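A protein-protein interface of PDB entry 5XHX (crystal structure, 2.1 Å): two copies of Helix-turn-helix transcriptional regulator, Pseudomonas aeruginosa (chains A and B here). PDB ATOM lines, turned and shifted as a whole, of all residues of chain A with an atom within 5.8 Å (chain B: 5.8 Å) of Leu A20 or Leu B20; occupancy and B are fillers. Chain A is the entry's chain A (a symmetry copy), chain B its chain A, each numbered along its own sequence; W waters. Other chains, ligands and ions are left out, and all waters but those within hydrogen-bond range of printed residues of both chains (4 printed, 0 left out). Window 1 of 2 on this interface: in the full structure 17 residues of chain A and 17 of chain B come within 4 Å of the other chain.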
ATOM      1  N   SER A  15     -15.640  11.459 -26.704  1.00  0.00           N
ATOM      2  CA  SER A  15     -16.695  10.610 -26.150  1.00  0.00           C
ATOM      3  C   SER A  15     -17.888  11.446 -25.728  1.00  0.00           C
ATOM      4  O   SER A  15     -19.042  11.118 -26.030  1.00  0.00           O
ATOM      5  CB  SER A  15     -16.175   9.815 -24.949  1.00  0.00           C
ATOM      6  OG  SER A  15     -15.277   8.807 -25.363  1.00  0.00           O
ATOM      7  N   LEU A  16     -17.626  12.537 -25.014  1.00  0.00           N
ATOM      8  CA  LEU A  16     -18.712  13.411 -24.595  1.00  0.00           C
ATOM      9  C   LEU A  16     -19.466  13.963 -25.802  1.00  0.00           C
ATOM     10  O   LEU A  16     -20.700  14.033 -25.795  1.00  0.00           O
ATOM     11  CB  LEU A  16     -18.149  14.530 -23.722  1.00  0.00           C
ATOM     12  CG  LEU A  16     -19.153  15.530 -23.156  1.00  0.00           C
ATOM     13  CD1 LEU A  16     -20.272  14.821 -22.383  1.00  0.00           C
ATOM     14  CD2 LEU A  16     -18.420  16.540 -22.277  1.00  0.00           C
ATOM     15  N   GLY A  17     -18.746  14.348 -26.858  1.00  0.00           N
ATOM     16  CA  GLY A  17     -19.424  14.889 -28.029  1.00  0.00           C
ATOM     17  C   GLY A  17     -20.332  13.872 -28.697  1.00  0.00           C
ATOM     18  O   GLY A  17     -21.446  14.194 -29.106  1.00  0.00           O
ATOM     19  N   LYS A  18     -19.869  12.624 -28.803  1.00  0.00           N
ATOM     20  CA  LYS A  18     -20.684  11.555 -29.378  1.00  0.00           C
ATOM     21  C   LYS A  18     -21.933  11.281 -28.538  1.00  0.00           C
ATOM     22  O   LYS A  18     -22.991  10.952 -29.079  1.00  0.00           O
ATOM     23  CB  LYS A  18     -19.801  10.305 -29.517  1.00  0.00           C
ATOM     24  CG  LYS A  18     -20.496   8.963 -29.700  1.00  0.00           C
ATOM     25  CD  LYS A  18     -19.473   7.816 -29.509  1.00  0.00           C
ATOM     26  CE  LYS A  18     -20.091   6.443 -29.754  1.00  0.00           C
ATOM     27  NZ  LYS A  18     -21.135   6.506 -30.806  1.00  0.00           N
ATOM     28  N   LEU A  19     -21.831  11.431 -27.222  1.00  0.00           N
ATOM     29  CA  LEU A  19     -22.973  11.219 -26.340  1.00  0.00           C
ATOM     30  C   LEU A  19     -23.988  12.342 -26.491  1.00  0.00           C
ATOM     31  O   LEU A  19     -25.195  12.097 -26.642  1.00  0.00           O
ATOM     32  CB  LEU A  19     -22.470  11.119 -24.903  1.00  0.00           C
ATOM     33  CG  LEU A  19     -23.491  10.993 -23.786  1.00  0.00           C
ATOM     34  CD1 LEU A  19     -24.325   9.733 -24.000  1.00  0.00           C
ATOM     35  CD2 LEU A  19     -22.741  10.946 -22.458  1.00  0.00           C
ATOM     36  N   LEU A  20     -23.504  13.592 -26.485  1.00  0.00           N
ATOM     37  CA  LEU A  20     -24.384  14.741 -26.665  1.00  0.00           C
ATOM     38  C   LEU A  20     -25.032  14.746 -28.042  1.00  0.00           C
ATOM     39  O   LEU A  20     -26.174  15.196 -28.183  1.00  0.00           O
ATOM     40  CB  LEU A  20     -23.594  16.041 -26.446  1.00  0.00           C
ATOM     41  CG  LEU A  20     -23.071  16.196 -25.021  1.00  0.00           C
ATOM     42  CD1 LEU A  20     -22.289  17.496 -24.825  1.00  0.00           C
ATOM     43  CD2 LEU A  20     -24.250  16.097 -24.041  1.00  0.00           C
ATOM     44  N   GLU A  21     -24.335  14.265 -29.050  1.00  0.00           N
ATOM     45  CA  GLU A  21     -24.867  14.218 -30.384  1.00  0.00           C
ATOM     46  C   GLU A  21     -26.022  13.212 -30.514  1.00  0.00           C
ATOM     47  O   GLU A  21     -26.915  13.381 -31.295  1.00  0.00           O
ATOM     48  CB  GLU A  21     -23.732  13.902 -31.350  1.00  0.00           C
ATOM     49  CG  GLU A  21     -24.058  13.972 -32.789  1.00  0.00           C
ATOM     50  CD  GLU A  21     -24.406  15.365 -33.255  1.00  0.00           C
ATOM     51  OE1 GLU A  21     -25.373  15.499 -34.014  1.00  0.00           O
ATOM     52  OE2 GLU A  21     -23.733  16.314 -32.857  1.00  0.00           O
ATOM     53  N   ALA A  22     -25.982  12.175 -29.696  1.00  0.00           N
ATOM     54  CA  ALA A  22     -26.982  11.113 -29.679  1.00  0.00           C
ATOM     55  C   ALA A  22     -28.238  11.488 -28.912  1.00  0.00           C
ATOM     56  O   ALA A  22     -29.185  10.695 -28.888  1.00  0.00           O
ATOM     57  CB  ALA A  22     -26.377   9.842 -29.073  1.00  0.00           C
ATOM     58  N   LEU A  23     -28.273  12.678 -28.309  1.00  0.00           N
ATOM     59  CA  LEU A  23     -29.339  13.028 -27.382  1.00  0.00           C
ATOM     60  C   LEU A  23     -30.715  12.967 -28.038  1.00  0.00           C
ATOM     61  O   LEU A  23     -31.710  12.714 -27.356  1.00  0.00           O
ATOM     62  CB  LEU A  23     -29.074  14.412 -26.789  1.00  0.00           C
ATOM     63  CG  LEU A  23     -29.979  14.949 -25.666  1.00  0.00           C
ATOM     64  CD1 LEU A  23     -30.070  13.993 -24.469  1.00  0.00           C
ATOM     65  CD2 LEU A  23     -29.480  16.323 -25.188  1.00  0.00           C
ATOM     66  N   ASP A  24     -30.797  13.174 -29.352  1.00  0.00           N
ATOM     67  CA  ASP A  24     -32.070  13.129 -30.063  1.00  0.00           C
ATOM     68  C   ASP A  24     -32.167  11.927 -30.989  1.00  0.00           C
ATOM     69  O   ASP A  24     -32.948  11.942 -31.938  1.00  0.00           O
ATOM     70  CB  ASP A  24     -32.293  14.421 -30.852  1.00  0.00           C
ATOM     71  CG  ASP A  24     -31.285  14.607 -31.986  1.00  0.00           C
ATOM     72  OD1 ASP A  24     -30.334  13.800 -32.110  1.00  0.00           O
ATOM     73  OD2 ASP A  24     -31.447  15.581 -32.754  1.00  0.00           O
ATOM     74  N   TRP A 165     -23.660  15.362 -14.409  1.00  0.00           N
ATOM     75  CA  TRP A 165     -24.039  15.492 -15.803  1.00  0.00           C
ATOM     76  C   TRP A 165     -24.797  14.281 -16.329  1.00  0.00           C
ATOM     77  O   TRP A 165     -25.526  14.419 -17.316  1.00  0.00           O
ATOM     78  CB  TRP A 165     -22.816  15.781 -16.692  1.00  0.00           C
ATOM     79  CG  TRP A 165     -21.697  14.779 -16.661  1.00  0.00           C
ATOM     80  CD1 TRP A 165     -20.549  14.871 -15.935  1.00  0.00           C
ATOM     81  CD2 TRP A 165     -21.603  13.565 -17.412  1.00  0.00           C
ATOM     82  NE1 TRP A 165     -19.751  13.771 -16.169  1.00  0.00           N
ATOM     83  CE2 TRP A 165     -20.368  12.964 -17.085  1.00  0.00           C
ATOM     84  CE3 TRP A 165     -22.435  12.934 -18.344  1.00  0.00           C
ATOM     85  CZ2 TRP A 165     -19.954  11.749 -17.637  1.00  0.00           C
ATOM     86  CZ3 TRP A 165     -22.028  11.729 -18.889  1.00  0.00           C
ATOM     87  CH2 TRP A 165     -20.796  11.148 -18.532  1.00  0.00           C
ATOM     88  N   ALA A 168     -28.350  15.327 -15.471  1.00  0.00           N
ATOM     89  CA  ALA A 168     -28.723  16.464 -16.309  1.00  0.00           C
ATOM     90  C   ALA A 168     -29.057  16.002 -17.717  1.00  0.00           C
ATOM     91  O   ALA A 168     -30.064  16.420 -18.307  1.00  0.00           O
ATOM     92  CB  ALA A 168     -27.587  17.496 -16.336  1.00  0.00           C
ATOM     93  N   LEU A 169     -28.213  15.136 -18.268  1.00  0.00           N
ATOM     94  CA  LEU A 169     -28.447  14.573 -19.592  1.00  0.00           C
ATOM     95  C   LEU A 169     -29.753  13.788 -19.638  1.00  0.00           C
ATOM     96  O   LEU A 169     -30.536  13.916 -20.583  1.00  0.00           O
ATOM     97  CB  LEU A 169     -27.287  13.644 -19.957  1.00  0.00           C
ATOM     98  CG  LEU A 169     -26.319  13.872 -21.100  1.00  0.00           C
ATOM     99  CD1 LEU A 169     -25.640  12.534 -21.378  1.00  0.00           C
ATOM    100  CD2 LEU A 169     -27.040  14.393 -22.325  1.00  0.00           C
ATOM    101  N   LYS A 172     -32.726  15.983 -19.830  1.00  0.00           N
ATOM    102  CA  LYS A 172     -32.880  16.618 -21.134  1.00  0.00           C
ATOM    103  C   LYS A 172     -33.326  15.618 -22.192  1.00  0.00           C
ATOM    104  O   LYS A 172     -34.069  15.980 -23.111  1.00  0.00           O
ATOM    105  CB  LYS A 172     -31.570  17.304 -21.542  1.00  0.00           C
ATOM    106  CG  LYS A 172     -31.254  18.540 -20.700  1.00  0.00           C
ATOM    107  CD  LYS A 172     -32.402  19.543 -20.787  1.00  0.00           C
ATOM    108  CE  LYS A 172     -32.146  20.777 -19.936  1.00  0.00           C
ATOM    109  NZ  LYS A 172     -32.588  20.618 -18.522  1.00  0.00           N
ATOM    110  N   SER B  15     -19.393  21.373 -13.413  1.00  0.00           N
ATOM    111  CA  SER B  15     -19.521  22.407 -14.440  1.00  0.00           C
ATOM    112  C   SER B  15     -20.280  21.877 -15.641  1.00  0.00           C
ATOM    113  O   SER B  15     -21.192  22.529 -16.164  1.00  0.00           O
ATOM    114  CB  SER B  15     -18.142  22.905 -14.882  1.00  0.00           C
ATOM    115  OG  SER B  15     -17.535  23.677 -13.867  1.00  0.00           O
ATOM    116  N   LEU B  16     -19.906  20.687 -16.102  1.00  0.00           N
ATOM    117  CA  LEU B  16     -20.604  20.092 -17.233  1.00  0.00           C
ATOM    118  C   LEU B  16     -22.084  19.890 -16.918  1.00  0.00           C
ATOM    119  O   LEU B  16     -22.948  20.150 -17.763  1.00  0.00           O
ATOM    120  CB  LEU B  16     -19.924  18.779 -17.609  1.00  0.00           C
ATOM    121  CG  LEU B  16     -20.499  18.026 -18.805  1.00  0.00           C
ATOM    122  CD1 LEU B  16     -20.561  18.920 -20.050  1.00  0.00           C
ATOM    123  CD2 LEU B  16     -19.668  16.770 -19.060  1.00  0.00           C
ATOM    124  N   GLY B  17     -22.402  19.442 -15.701  1.00  0.00           N
ATOM    125  CA  GLY B  17     -23.802  19.227 -15.360  1.00  0.00           C
ATOM    126  C   GLY B  17     -24.609  20.514 -15.377  1.00  0.00           C
ATOM    127  O   GLY B  17     -25.738  20.543 -15.863  1.00  0.00           O
ATOM    128  N   LYS B  18     -24.031  21.598 -14.855  1.00  0.00           N
ATOM    129  CA  LYS B  18     -24.698  22.900 -14.872  1.00  0.00           C
ATOM    130  C   LYS B  18     -24.919  23.404 -16.299  1.00  0.00           C
ATOM    131  O   LYS B  18     -25.926  24.057 -16.582  1.00  0.00           O
ATOM    132  CB  LYS B  18     -23.852  23.879 -14.042  1.00  0.00           C
ATOM    133  CG  LYS B  18     -24.099  25.368 -14.236  1.00  0.00           C
ATOM    134  CD  LYS B  18     -22.961  26.177 -13.564  1.00  0.00           C
ATOM    135  CE  LYS B  18     -23.188  27.682 -13.656  1.00  0.00           C
ATOM    136  NZ  LYS B  18     -24.635  28.009 -13.599  1.00  0.00           N
ATOM    137  N   LEU B  19     -24.001  23.094 -17.208  1.00  0.00           N
ATOM    138  CA  LEU B  19     -24.137  23.506 -18.599  1.00  0.00           C
ATOM    139  C   LEU B  19     -25.236  22.715 -19.293  1.00  0.00           C
ATOM    140  O   LEU B  19     -26.105  23.285 -19.971  1.00  0.00           O
ATOM    141  CB  LEU B  19     -22.795  23.317 -19.300  1.00  0.00           C
ATOM    142  CG  LEU B  19     -22.711  23.590 -20.792  1.00  0.00           C
ATOM    143  CD1 LEU B  19     -23.097  25.041 -21.064  1.00  0.00           C
ATOM    144  CD2 LEU B  19     -21.287  23.296 -21.251  1.00  0.00           C
ATOM    145  N   LEU B  20     -25.229  21.388 -19.103  1.00  0.00           N
ATOM    146  CA  LEU B  20     -26.262  20.539 -19.687  1.00  0.00           C
ATOM    147  C   LEU B  20     -27.638  20.851 -19.118  1.00  0.00           C
ATOM    148  O   LEU B  20     -28.639  20.737 -19.832  1.00  0.00           O
ATOM    149  CB  LEU B  20     -25.914  19.061 -19.451  1.00  0.00           C
ATOM    150  CG  LEU B  20     -24.633  18.622 -20.156  1.00  0.00           C
ATOM    151  CD1 LEU B  20     -24.306  17.149 -19.909  1.00  0.00           C
ATOM    152  CD2 LEU B  20     -24.759  18.926 -21.656  1.00  0.00           C
ATOM    153  N   GLU B  21     -27.710  21.234 -17.860  1.00  0.00           N
ATOM    154  CA  GLU B  21     -28.964  21.561 -17.240  1.00  0.00           C
ATOM    155  C   GLU B  21     -29.581  22.845 -17.817  1.00  0.00           C
ATOM    156  O   GLU B  21     -30.769  23.002 -17.867  1.00  0.00           O
ATOM    157  CB  GLU B  21     -28.750  21.666 -15.735  1.00  0.00           C
ATOM    158  CG  GLU B  21     -29.963  21.837 -14.910  1.00  0.00           C
ATOM    159  CD  GLU B  21     -30.887  20.643 -14.952  1.00  0.00           C
ATOM    160  OE1 GLU B  21     -32.100  20.851 -15.064  1.00  0.00           O
ATOM    161  OE2 GLU B  21     -30.406  19.513 -14.889  1.00  0.00           O
ATOM    162  N   ALA B  22     -28.728  23.742 -18.278  1.00  0.00           N
ATOM    163  CA  ALA B  22     -29.124  25.023 -18.852  1.00  0.00           C
ATOM    164  C   ALA B  22     -29.571  24.915 -20.300  1.00  0.00           C
ATOM    165  O   ALA B  22     -29.997  25.924 -20.872  1.00  0.00           O
ATOM    166  CB  ALA B  22     -27.962  26.017 -18.753  1.00  0.00           C
ATOM    167  N   LEU B  23     -29.503  23.719 -20.890  1.00  0.00           N
ATOM    168  CA  LEU B  23     -29.707  23.569 -22.324  1.00  0.00           C
ATOM    169  C   LEU B  23     -31.081  24.061 -22.766  1.00  0.00           C
ATOM    170  O   LEU B  23     -31.240  24.495 -23.909  1.00  0.00           O
ATOM    171  CB  LEU B  23     -29.490  22.109 -22.725  1.00  0.00           C
ATOM    172  CG  LEU B  23     -29.499  21.715 -24.213  1.00  0.00           C
ATOM    173  CD1 LEU B  23     -28.500  22.529 -25.047  1.00  0.00           C
ATOM    174  CD2 LEU B  23     -29.196  20.216 -24.370  1.00  0.00           C
ATOM    175  N   ASP B  24     -32.078  24.024 -21.882  1.00  0.00           N
ATOM    176  CA  ASP B  24     -33.422  24.479 -22.217  1.00  0.00           C
ATOM    177  C   ASP B  24     -33.796  25.755 -21.479  1.00  0.00           C
ATOM    178  O   ASP B  24     -34.979  26.048 -21.314  1.00  0.00           O
ATOM    179  CB  ASP B  24     -34.451  23.383 -21.927  1.00  0.00           C
ATOM    180  CG  ASP B  24     -34.571  23.057 -20.439  1.00  0.00           C
ATOM    181  OD1 ASP B  24     -33.785  23.592 -19.621  1.00  0.00           O
ATOM    182  OD2 ASP B  24     -35.458  22.249 -20.090  1.00  0.00           O
ATOM    183  N   TRP B 165     -17.660  18.455 -28.219  1.00  0.00           N
ATOM    184  CA  TRP B 165     -18.897  18.579 -27.470  1.00  0.00           C
ATOM    185  C   TRP B 165     -19.453  19.995 -27.469  1.00  0.00           C
ATOM    186  O   TRP B 165     -20.657  20.162 -27.254  1.00  0.00           O
ATOM    187  CB  TRP B 165     -18.730  18.072 -26.026  1.00  0.00           C
ATOM    188  CG  TRP B 165     -17.673  18.732 -25.188  1.00  0.00           C
ATOM    189  CD1 TRP B 165     -16.416  18.264 -24.953  1.00  0.00           C
ATOM    190  CD2 TRP B 165     -17.793  19.951 -24.448  1.00  0.00           C
ATOM    191  NE1 TRP B 165     -15.733  19.131 -24.128  1.00  0.00           N
ATOM    192  CE2 TRP B 165     -16.562  20.165 -23.789  1.00  0.00           C
ATOM    193  CE3 TRP B 165     -18.827  20.875 -24.261  1.00  0.00           C
ATOM    194  CZ2 TRP B 165     -16.327  21.278 -22.978  1.00  0.00           C
ATOM    195  CZ3 TRP B 165     -18.595  21.979 -23.461  1.00  0.00           C
ATOM    196  CH2 TRP B 165     -17.352  22.172 -22.829  1.00  0.00           C
ATOM    197  N   ALA B 168     -21.600  19.844 -30.603  1.00  0.00           N
ATOM    198  CA  ALA B 168     -22.723  18.941 -30.362  1.00  0.00           C
ATOM    199  C   ALA B 168     -23.780  19.621 -29.510  1.00  0.00           C
ATOM    200  O   ALA B 168     -24.983  19.549 -29.802  1.00  0.00           O
ATOM    201  CB  ALA B 168     -22.232  17.654 -29.685  1.00  0.00           C
ATOM    202  N   LEU B 169     -23.341  20.286 -28.446  1.00  0.00           N
ATOM    203  CA  LEU B 169     -24.246  21.028 -27.578  1.00  0.00           C
ATOM    204  C   LEU B 169     -24.970  22.131 -28.342  1.00  0.00           C
ATOM    205  O   LEU B 169     -26.181  22.316 -28.192  1.00  0.00           O
ATOM    206  CB  LEU B 169     -23.447  21.649 -26.430  1.00  0.00           C
ATOM    207  CG  LEU B 169     -23.611  21.296 -24.966  1.00  0.00           C
ATOM    208  CD1 LEU B 169     -22.977  22.428 -24.163  1.00  0.00           C
ATOM    209  CD2 LEU B 169     -25.073  21.117 -24.613  1.00  0.00           C
ATOM    210  N   LYS B 172     -27.729  20.835 -30.439  1.00  0.00           N
ATOM    211  CA  LYS B 172     -28.883  20.405 -29.656  1.00  0.00           C
ATOM    212  C   LYS B 172     -29.639  21.593 -29.079  1.00  0.00           C
ATOM    213  O   LYS B 172     -30.867  21.540 -28.947  1.00  0.00           O
ATOM    214  CB  LYS B 172     -28.437  19.443 -28.547  1.00  0.00           C
ATOM    215  CG  LYS B 172     -27.979  18.086 -29.081  1.00  0.00           C
ATOM    216  CD  LYS B 172     -29.094  17.438 -29.897  1.00  0.00           C
ATOM    217  CE  LYS B 172     -28.671  16.098 -30.477  1.00  0.00           C
ATOM    218  NZ  LYS B 172     -27.980  16.218 -31.792  1.00  0.00           N
HETATM  219  O   HOH W   1     -31.009  18.837 -17.263  1.00  0.00           O
HETATM  220  O   HOH W   2     -29.797  17.758 -33.583  1.00  0.00           O
HETATM  221  O   HOH W   3     -25.571  17.373 -31.458  1.00  0.00           O
HETATM  222  O   HOH W   4     -35.457  19.812 -18.602  1.00  0.00           O
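Of the 14 printed residues of chain A, 9 touch a printed residue of chain B. Printed residues of chain A that touch a printed residue of chain B: Leu A16, Gly A17, Leu A20, Glu A21, Leu A23, Asp A24, Trp A165, Ala A168 and Lys A172. Hydrophobic or aromatic side chains of chain A within 4 Å of the printed part of chain B: Leu A16, Leu A20, Leu A23, Trp A165 and Ala A168. Among the printed residues, Asp or Glu carboxylates within 4 Å of a Lys or Arg side-chain nitrogen of the other chain: Glu A21 with Lys B172, Asp A24 with Lys B172, Lys A172 with Glu B21 and Lys A172 with Asp B24.
Leu A16 touches its own counterpart, Leu B16. Gly A17 touches Ala B168, and with the chains exchanged Ala A168 touches Gly B17. Leu A20 touches its own counterpart, Leu B20. Glu A21 touches Lys B172, and with the chains exchanged Lys A172 touches Glu B21. Positions printed for both chains: 15, 16, 17, 18, 19, 20, 21, 22, 23, 24, 165, 168, 169 and 172. Of the 21 pairs that touch across the chains among the printed residues, 21 have their exchanged pair printed and touching as well.
Of chain B, only Leu B20 (3.7 Å), Trp B165 (3.8 Å), Ala B168 (3.9 Å) and Lys B172 (3.5 Å) come within 4 Å of Leu A20. Of the printed residues of chain A, Lys B172 touches Leu A20 (3.5 Å), Glu A21 (3.1 Å) and Asp A24 (3.3 Å). Printed residues of chain A within 4 Å of Leu B16: Leu A16 and Trp A165. Of the printed residues of chain A, Trp B165 touches Leu A16 (3.7 Å), Gly A17 (3.8 Å) and Leu A20 (3.8 Å). Printed residues of chain B within 4 Å of Trp A165: Leu B16, Gly B17 and Leu B20. Of the printed residues of chain B, Glu A21 touches Ala B168 (3.8 Å) and Lys B172 (3.1 Å). Ala B22 touches none of the printed residues of chain A. Leu B19 touches none of the printed residues of chain A. The nearest printed residue of chain A that does not touch Glu B21 is Leu A169 (5.9 Å).
Water W1 lies within hydrogen-bond range of OE2 of Glu B21, NZ of Lys A172 and O of Ala A168. Water W3 lies within hydrogen-bond range of the side-chain carboxylate of Glu A21 (2.5 Å), the side-chain amino group of Lys B172 (2.7 Å) and the backbone carbonyl oxygen of Ala B168 (2.8 Å). Water W4 lies within hydrogen-bond range of the side-chain carboxylate (OD2) of Asp B24 (2.9 Å) and the side-chain amino group (NZ) of Lys A172 (3.0 Å). Water W2 bridges OD2 of Asp A24 (2.9 Å) and NZ of Lys B172 (3.0 Å).
Among the printed residues, merely in contact across the chains: Leu A16 with Leu B16 (3.5 Å), Leu A16 with Trp B165 (3.7 Å), Gly A17 with Trp B165 (3.8 Å), Gly A17 with Ala B168 (3.6 Å), Leu A20 with Leu B20 (3.7 Å), Leu A20 with Trp B165 (3.8 Å), Leu A20 with Ala B168 (3.9 Å), Leu A20 with Lys B172 (3.5 Å), Glu A21 with Ala B168 (3.8 Å), Leu A23 with Leu B23 (3.99 Å), Trp A165 with Leu B16 (3.7 Å), Trp A165 with Gly B17 (3.8 Å), Trp A165 with Leu B20 (3.8 Å), Ala A168 with Gly B17 (3.6 Å), Ala A168 with Leu B20 (3.9 Å), Ala A168 with Glu B21 (3.8 Å) and Lys A172 with Leu B20 (3.5 Å).
NZ of Lys A172 is in salt-bridge range of OD1 of Asp B24 (3.4 Å). NZ of Lys A172 is in salt-bridge range of OE1 of Glu B21 (3.5 Å). The side-chain amino group (NZ) of Lys B172 lies within salt-bridge range of the side-chain carboxylate (OE1) of Glu A21 (3.5 Å). The side-chain amino group of Lys B172 is in salt-bridge range of the side-chain carboxylate of Asp A24 (3.4 Å).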
